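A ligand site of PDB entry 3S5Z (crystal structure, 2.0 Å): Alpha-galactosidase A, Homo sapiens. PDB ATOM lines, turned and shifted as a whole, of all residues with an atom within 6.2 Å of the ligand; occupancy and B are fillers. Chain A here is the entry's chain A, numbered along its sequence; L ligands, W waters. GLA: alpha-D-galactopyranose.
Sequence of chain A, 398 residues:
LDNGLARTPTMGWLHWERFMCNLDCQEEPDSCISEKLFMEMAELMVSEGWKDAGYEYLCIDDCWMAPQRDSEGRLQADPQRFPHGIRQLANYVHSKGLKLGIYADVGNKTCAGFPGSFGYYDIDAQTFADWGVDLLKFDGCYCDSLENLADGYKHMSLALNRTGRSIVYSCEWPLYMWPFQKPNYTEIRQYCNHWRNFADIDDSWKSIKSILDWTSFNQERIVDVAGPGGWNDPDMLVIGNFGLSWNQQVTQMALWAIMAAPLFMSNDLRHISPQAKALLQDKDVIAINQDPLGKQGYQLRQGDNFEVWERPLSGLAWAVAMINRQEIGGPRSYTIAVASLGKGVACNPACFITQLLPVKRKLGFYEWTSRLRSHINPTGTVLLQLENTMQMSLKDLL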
ATOM      1  N   LEU A  14       9.348 -16.520  20.506  1.00  0.00           N
ATOM      2  CA  LEU A  14      10.330 -16.766  19.453  1.00  0.00           C
ATOM      3  C   LEU A  14       9.699 -17.746  18.457  1.00  0.00           C
ATOM      4  O   LEU A  14       9.159 -18.772  18.858  1.00  0.00           O
ATOM      5  CB  LEU A  14      11.592 -17.345  20.086  1.00  0.00           C
ATOM      6  CG  LEU A  14      12.863 -17.543  19.276  1.00  0.00           C
ATOM      7  CD1 LEU A  14      13.278 -16.270  18.534  1.00  0.00           C
ATOM      8  CD2 LEU A  14      13.979 -17.992  20.228  1.00  0.00           C
ATOM      9  N   TRP A  16      10.756 -19.853  16.199  1.00  0.00           N
ATOM     10  CA  TRP A  16      11.451 -20.951  15.545  1.00  0.00           C
ATOM     11  C   TRP A  16      10.822 -22.338  15.707  1.00  0.00           C
ATOM     12  O   TRP A  16      10.528 -22.990  14.717  1.00  0.00           O
ATOM     13  CB  TRP A  16      12.912 -21.020  15.949  1.00  0.00           C
ATOM     14  CG  TRP A  16      13.614 -22.092  15.179  1.00  0.00           C
ATOM     15  CD1 TRP A  16      14.062 -23.292  15.651  1.00  0.00           C
ATOM     16  CD2 TRP A  16      13.873 -22.095  13.776  1.00  0.00           C
ATOM     17  NE1 TRP A  16      14.626 -24.019  14.636  1.00  0.00           N
ATOM     18  CE2 TRP A  16      14.518 -23.312  13.468  1.00  0.00           C
ATOM     19  CE3 TRP A  16      13.656 -21.172  12.743  1.00  0.00           C
ATOM     20  CZ2 TRP A  16      14.924 -23.641  12.181  1.00  0.00           C
ATOM     21  CZ3 TRP A  16      14.061 -21.494  11.468  1.00  0.00           C
ATOM     22  CH2 TRP A  16      14.690 -22.715  11.186  1.00  0.00           C
ATOM     23  N   ASP A  61      13.255 -15.257  14.449  1.00  0.00           N
ATOM     24  CA  ASP A  61      14.382 -16.193  14.322  1.00  0.00           C
ATOM     25  C   ASP A  61      14.849 -16.213  12.856  1.00  0.00           C
ATOM     26  O   ASP A  61      14.625 -15.255  12.129  1.00  0.00           O
ATOM     27  CB  ASP A  61      13.984 -17.583  14.853  1.00  0.00           C
ATOM     28  CG  ASP A  61      15.181 -18.366  15.430  1.00  0.00           C
ATOM     29  OD1 ASP A  61      15.931 -18.975  14.650  1.00  0.00           O
ATOM     30  OD2 ASP A  61      15.339 -18.397  16.665  1.00  0.00           O
ATOM     31  N   ASP A  62      15.526 -17.275  12.438  1.00  0.00           N
ATOM     32  CA  ASP A  62      16.117 -17.397  11.103  1.00  0.00           C
ATOM     33  C   ASP A  62      15.039 -17.314  10.025  1.00  0.00           C
ATOM     34  O   ASP A  62      13.841 -17.422  10.315  1.00  0.00           O
ATOM     35  CB  ASP A  62      16.882 -18.742  11.027  1.00  0.00           C
ATOM     36  CG  ASP A  62      17.986 -18.769   9.969  1.00  0.00           C
ATOM     37  OD1 ASP A  62      18.139 -17.824   9.165  1.00  0.00           O
ATOM     38  OD2 ASP A  62      18.728 -19.769   9.949  1.00  0.00           O
ATOM     39  N   CYS A  63      15.470 -17.081   8.782  1.00  0.00           N
ATOM     40  CA  CYS A  63      14.582 -17.007   7.600  1.00  0.00           C
ATOM     41  C   CYS A  63      13.718 -15.755   7.495  1.00  0.00           C
ATOM     42  O   CYS A  63      12.625 -15.788   6.918  1.00  0.00           O
ATOM     43  CB  CYS A  63      13.734 -18.295   7.461  1.00  0.00           C
ATOM     44  SG  CYS A  63      14.750 -19.793   7.615  1.00  0.00           S
ATOM     45  N   TYR A 103      17.415 -12.164  14.498  1.00  0.00           N
ATOM     46  CA  TYR A 103      18.400 -13.226  14.441  1.00  0.00           C
ATOM     47  C   TYR A 103      19.485 -12.930  13.403  1.00  0.00           C
ATOM     48  O   TYR A 103      19.214 -12.370  12.340  1.00  0.00           O
ATOM     49  CB  TYR A 103      17.681 -14.534  14.078  1.00  0.00           C
ATOM     50  CG  TYR A 103      18.561 -15.722  13.699  1.00  0.00           C
ATOM     51  CD1 TYR A 103      18.780 -16.778  14.588  1.00  0.00           C
ATOM     52  CD2 TYR A 103      19.119 -15.806  12.428  1.00  0.00           C
ATOM     53  CE1 TYR A 103      19.581 -17.872  14.215  1.00  0.00           C
ATOM     54  CE2 TYR A 103      19.900 -16.877  12.063  1.00  0.00           C
ATOM     55  CZ  TYR A 103      20.132 -17.913  12.950  1.00  0.00           C
ATOM     56  OH  TYR A 103      20.928 -18.980  12.559  1.00  0.00           O
ATOM     57  N   THR A 110      23.568 -18.046   7.806  1.00  0.00           N
ATOM     58  CA  THR A 110      22.685 -18.505   8.880  1.00  0.00           C
ATOM     59  C   THR A 110      22.519 -20.013   8.750  1.00  0.00           C
ATOM     60  O   THR A 110      22.791 -20.585   7.692  1.00  0.00           O
ATOM     61  CB  THR A 110      21.309 -17.831   8.837  1.00  0.00           C
ATOM     62  OG1 THR A 110      20.560 -18.311   7.729  1.00  0.00           O
ATOM     63  CG2 THR A 110      21.439 -16.299   8.753  1.00  0.00           C
ATOM     64  N   CYS A 111      22.061 -20.674   9.806  1.00  0.00           N
ATOM     65  CA  CYS A 111      21.919 -22.127   9.746  1.00  0.00           C
ATOM     66  C   CYS A 111      20.964 -22.543   8.621  1.00  0.00           C
ATOM     67  O   CYS A 111      21.181 -23.581   8.018  1.00  0.00           O
ATOM     68  CB  CYS A 111      21.475 -22.710  11.091  1.00  0.00           C
ATOM     69  SG  CYS A 111      22.588 -22.312  12.450  1.00  0.00           S
ATOM     70  N   ALA A 112      19.964 -21.718   8.322  1.00  0.00           N
ATOM     71  CA  ALA A 112      19.047 -21.987   7.201  1.00  0.00           C
ATOM     72  C   ALA A 112      19.617 -21.572   5.836  1.00  0.00           C
ATOM     73  O   ALA A 112      18.966 -21.792   4.820  1.00  0.00           O
ATOM     74  CB  ALA A 112      17.703 -21.311   7.431  1.00  0.00           C
ATOM     75  N   LYS A 137      19.676 -12.459  18.660  1.00  0.00           N
ATOM     76  CA  LYS A 137      20.061 -13.843  18.861  1.00  0.00           C
ATOM     77  C   LYS A 137      21.103 -14.129  17.799  1.00  0.00           C
ATOM     78  O   LYS A 137      20.834 -13.978  16.599  1.00  0.00           O
ATOM     79  CB  LYS A 137      18.846 -14.776  18.726  1.00  0.00           C
ATOM     80  CG  LYS A 137      19.205 -16.260  18.718  1.00  0.00           C
ATOM     81  CD  LYS A 137      17.966 -17.166  18.698  1.00  0.00           C
ATOM     82  CE  LYS A 137      18.339 -18.615  18.384  1.00  0.00           C
ATOM     83  NZ  LYS A 137      17.160 -19.534  18.296  1.00  0.00           N
ATOM     84  N   ASP A 139      23.789 -16.708  16.171  1.00  0.00           N
ATOM     85  CA  ASP A 139      23.986 -18.120  16.019  1.00  0.00           C
ATOM     86  C   ASP A 139      25.395 -18.406  15.519  1.00  0.00           C
ATOM     87  O   ASP A 139      26.094 -17.500  15.098  1.00  0.00           O
ATOM     88  CB  ASP A 139      22.938 -18.641  15.050  1.00  0.00           C
ATOM     89  CG  ASP A 139      22.675 -20.124  15.194  1.00  0.00           C
ATOM     90  OD1 ASP A 139      23.402 -20.831  15.939  1.00  0.00           O
ATOM     91  OD2 ASP A 139      21.708 -20.558  14.550  1.00  0.00           O
ATOM     92  N   CYS A 141      26.518 -21.073  13.236  1.00  0.00           N
ATOM     93  CA  CYS A 141      26.698 -21.898  12.039  1.00  0.00           C
ATOM     94  C   CYS A 141      27.696 -21.308  11.057  1.00  0.00           C
ATOM     95  O   CYS A 141      27.961 -20.108  11.074  1.00  0.00           O
ATOM     96  CB  CYS A 141      25.358 -22.088  11.310  1.00  0.00           C
ATOM     97  SG  CYS A 141      24.292 -23.333  12.023  1.00  0.00           S
ATOM     98  N   GLU A 172      25.148 -18.298  21.065  1.00  0.00           N
ATOM     99  CA  GLU A 172      25.157 -19.767  21.010  1.00  0.00           C
ATOM    100  C   GLU A 172      26.590 -20.258  21.070  1.00  0.00           C
ATOM    101  O   GLU A 172      26.901 -21.408  20.752  1.00  0.00           O
ATOM    102  CB  GLU A 172      24.440 -20.266  19.766  1.00  0.00           C
ATOM    103  CG  GLU A 172      22.995 -19.757  19.709  1.00  0.00           C
ATOM    104  CD  GLU A 172      22.076 -20.598  18.815  1.00  0.00           C
ATOM    105  OE1 GLU A 172      21.011 -20.185  18.456  1.00  0.00           O
ATOM    106  OE2 GLU A 172      22.364 -21.691  18.433  1.00  0.00           O
ATOM    107  N   LEU A 175      27.597 -23.748  22.819  1.00  0.00           N
ATOM    108  CA  LEU A 175      27.069 -24.850  22.014  1.00  0.00           C
ATOM    109  C   LEU A 175      27.975 -25.208  20.846  1.00  0.00           C
ATOM    110  O   LEU A 175      28.245 -26.383  20.605  1.00  0.00           O
ATOM    111  CB  LEU A 175      25.668 -24.527  21.500  1.00  0.00           C
ATOM    112  CG  LEU A 175      25.082 -25.487  20.464  1.00  0.00           C
ATOM    113  CD1 LEU A 175      25.063 -26.938  20.983  1.00  0.00           C
ATOM    114  CD2 LEU A 175      23.696 -25.011  20.074  1.00  0.00           C
ATOM    115  N   TYR A 176      28.424 -24.208  20.095  1.00  0.00           N
ATOM    116  CA  TYR A 176      29.263 -24.477  18.912  1.00  0.00           C
ATOM    117  C   TYR A 176      30.726 -24.741  19.296  1.00  0.00           C
ATOM    118  O   TYR A 176      31.525 -25.230  18.482  1.00  0.00           O
ATOM    119  CB  TYR A 176      29.125 -23.349  17.887  1.00  0.00           C
ATOM    120  CG  TYR A 176      27.773 -23.375  17.220  1.00  0.00           C
ATOM    121  CD1 TYR A 176      27.561 -24.047  16.018  1.00  0.00           C
ATOM    122  CD2 TYR A 176      26.669 -22.737  17.808  1.00  0.00           C
ATOM    123  CE1 TYR A 176      26.310 -24.104  15.426  1.00  0.00           C
ATOM    124  CE2 TYR A 176      25.433 -22.780  17.227  1.00  0.00           C
ATOM    125  CZ  TYR A 176      25.248 -23.458  16.032  1.00  0.00           C
ATOM    126  OH  TYR A 176      24.004 -23.473  15.474  1.00  0.00           O
ATOM    127  N   ARG A 196      23.198 -20.299  24.757  1.00  0.00           N
ATOM    128  CA  ARG A 196      22.687 -21.636  24.516  1.00  0.00           C
ATOM    129  C   ARG A 196      23.828 -22.626  24.745  1.00  0.00           C
ATOM    130  O   ARG A 196      24.905 -22.460  24.167  1.00  0.00           O
ATOM    131  CB  ARG A 196      22.154 -21.755  23.082  1.00  0.00           C
ATOM    132  CG  ARG A 196      20.783 -21.103  22.860  1.00  0.00           C
ATOM    133  CD  ARG A 196      19.645 -22.069  23.195  1.00  0.00           C
ATOM    134  NE  ARG A 196      19.929 -23.369  22.581  1.00  0.00           N
ATOM    135  CZ  ARG A 196      19.704 -23.669  21.301  1.00  0.00           C
ATOM    136  NH1 ARG A 196      19.156 -22.787  20.470  1.00  0.00           N
ATOM    137  NH2 ARG A 196      20.030 -24.872  20.859  1.00  0.00           N
ATOM    138  N   ASP A 200      19.370 -28.077  19.885  1.00  0.00           N
ATOM    139  CA  ASP A 200      18.039 -27.475  19.725  1.00  0.00           C
ATOM    140  C   ASP A 200      16.957 -28.319  20.368  1.00  0.00           C
ATOM    141  O   ASP A 200      16.930 -29.536  20.200  1.00  0.00           O
ATOM    142  CB  ASP A 200      17.691 -27.319  18.234  1.00  0.00           C
ATOM    143  CG  ASP A 200      18.545 -26.287  17.501  1.00  0.00           C
ATOM    144  OD1 ASP A 200      19.420 -25.653  18.116  1.00  0.00           O
ATOM    145  OD2 ASP A 200      18.325 -26.105  16.280  1.00  0.00           O
ATOM    146  N   ASP A 235      17.002 -23.346  25.943  1.00  0.00           N
ATOM    147  CA  ASP A 235      16.162 -23.258  24.733  1.00  0.00           C
ATOM    148  C   ASP A 235      14.680 -23.011  25.056  1.00  0.00           C
ATOM    149  O   ASP A 235      14.315 -22.853  26.221  1.00  0.00           O
ATOM    150  CB  ASP A 235      16.366 -24.466  23.789  1.00  0.00           C
ATOM    151  CG  ASP A 235      16.257 -24.088  22.308  1.00  0.00           C
ATOM    152  OD1 ASP A 235      15.869 -22.940  22.011  1.00  0.00           O
ATOM    153  OD2 ASP A 235      16.561 -24.938  21.437  1.00  0.00           O
ATOM    154  N   MET A 236      13.849 -22.949  24.015  1.00  0.00           N
ATOM    155  CA  MET A 236      12.470 -22.479  24.100  1.00  0.00           C
ATOM    156  C   MET A 236      11.533 -23.323  24.957  1.00  0.00           C
ATOM    157  O   MET A 236      11.703 -24.528  25.101  1.00  0.00           O
ATOM    158  CB  MET A 236      11.888 -22.389  22.680  1.00  0.00           C
ATOM    159  CG  MET A 236      12.501 -21.287  21.812  1.00  0.00           C
ATOM    160  SD  MET A 236      12.301 -21.484  20.016  1.00  0.00           S
ATOM    161  CE  MET A 236      13.586 -22.720  19.704  1.00  0.00           C
HETATM  162  C1  GLA L   1      20.180 -23.110  15.002  1.00  0.00           C
HETATM  163  C2  GLA L   1      19.720 -22.564  16.356  1.00  0.00           C
HETATM  164  C3  GLA L   1      18.202 -22.660  16.486  1.00  0.00           C
HETATM  165  C4  GLA L   1      17.579 -21.861  15.361  1.00  0.00           C
HETATM  166  C5  GLA L   1      18.117 -22.329  14.002  1.00  0.00           C
HETATM  167  C6  GLA L   1      17.687 -21.369  12.901  1.00  0.00           C
HETATM  168  O1  GLA L   1      19.900 -24.483  14.907  1.00  0.00           O
HETATM  169  O2  GLA L   1      20.399 -23.283  17.362  1.00  0.00           O
HETATM  170  O3  GLA L   1      17.750 -22.147  17.727  1.00  0.00           O
HETATM  171  O4  GLA L   1      17.834 -20.477  15.563  1.00  0.00           O
HETATM  172  O5  GLA L   1      19.540 -22.403  13.958  1.00  0.00           O
HETATM  173  O6  GLA L   1      18.007 -21.861  11.613  1.00  0.00           O
HETATM  174  O   HOH W   1      17.844 -24.095  10.470  1.00  0.00           O
HETATM  175  O   HOH W   2      17.518 -20.731  20.883  1.00  0.00           O
HETATM  176  O   HOH W   3      16.097 -24.146  18.923  1.00  0.00           O
HETATM  177  O   HOH W   4      22.466 -25.786  16.017  1.00  0.00           O
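O5 of the ligand lies close to SG of Cys 111, 3.4 Å away.
An oxygen (O5) of the ligand sits close to the side-chain carboxylate (OD2) of Asp 139, 2.9 Å away.
Merely in contact with the ligand: Tyr 103 (3.4 Å), Trp 16 (3.5 Å), Ala 112 (3.8 Å) and Tyr 176 (3.9 Å).
Hydrophobic or aromatic side chains within 4 Å of the ligand: Trp 16 and Tyr 103.
The nearest printed residue that does not touch the ligand is Leu 175 (4.6 Å).
Water W3 bridges the side-chain carboxylate (OD2) of Asp 235 (2.7 Å) and an oxygen (O3) of the ligand (2.9 Å).
Water W4 lies within hydrogen-bond range of OH of Tyr 176 (2.8 Å) and O1 of the ligand (3.1 Å).
Water W2 lies within hydrogen-bond range of NH1 of Arg 196 (2.7 Å), NZ of Lys 137 (2.9 Å), OD1 of Asp 235 (3.0 Å) and O3 of the ligand (3.5 Å).
The side-chain carboxylate of Asp 61 is in hydrogen-bond range of an oxygen (O4) of the ligand.
OD2 of Asp 200 is in hydrogen-bond range of O1 of the ligand (2.6 Å).
NZ of Lys 137 lies within hydrogen-bond range of O3 of the ligand (2.7 Å).
An oxygen (O2) of the ligand sits at hydrogen-bond distance from the side-chain carboxylate (OE2) of Glu 172 (2.7 Å).
An oxygen (O6) of the ligand is in hydrogen-bond range of the side-chain carboxylate of Asp 62 (2.8 Å).
The guanidinium group of Arg 196 is in hydrogen-bond range of an oxygen (O3) of the ligand, at 3.1 Å.
The side-chain carboxylate (OD2) of Asp 61 lies within salt-bridge range of the side-chain amino group (NZ) of Lys 137 (2.7 Å).
The side-chain carboxylate (OD1) of Asp 200 is in salt-bridge range of the guanidinium group (NH2) of Arg 196, at 2.9 Å.
NZ of Lys 137 lies within salt-bridge range of OE1 of Glu 172, at 3.9 Å.
The side-chain carboxylate of Glu 172 lies within salt-bridge range of the guanidinium group of Arg 196 (3.8 Å).
N of Ala 112 sits at hydrogen-bond distance from OD2 of Asp 62.
The side-chain hydroxyl of Thr 110 is in hydrogen-bond range of the side-chain carboxylate of Asp 62 (2.9 Å).
The backbone NH (N) of Leu 175 is in hydrogen-bond range of the backbone carbonyl oxygen (O) of Arg 196.
SG of Cys 141 forms a disulfide with SG of Cys 111, at 2.0 Å.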
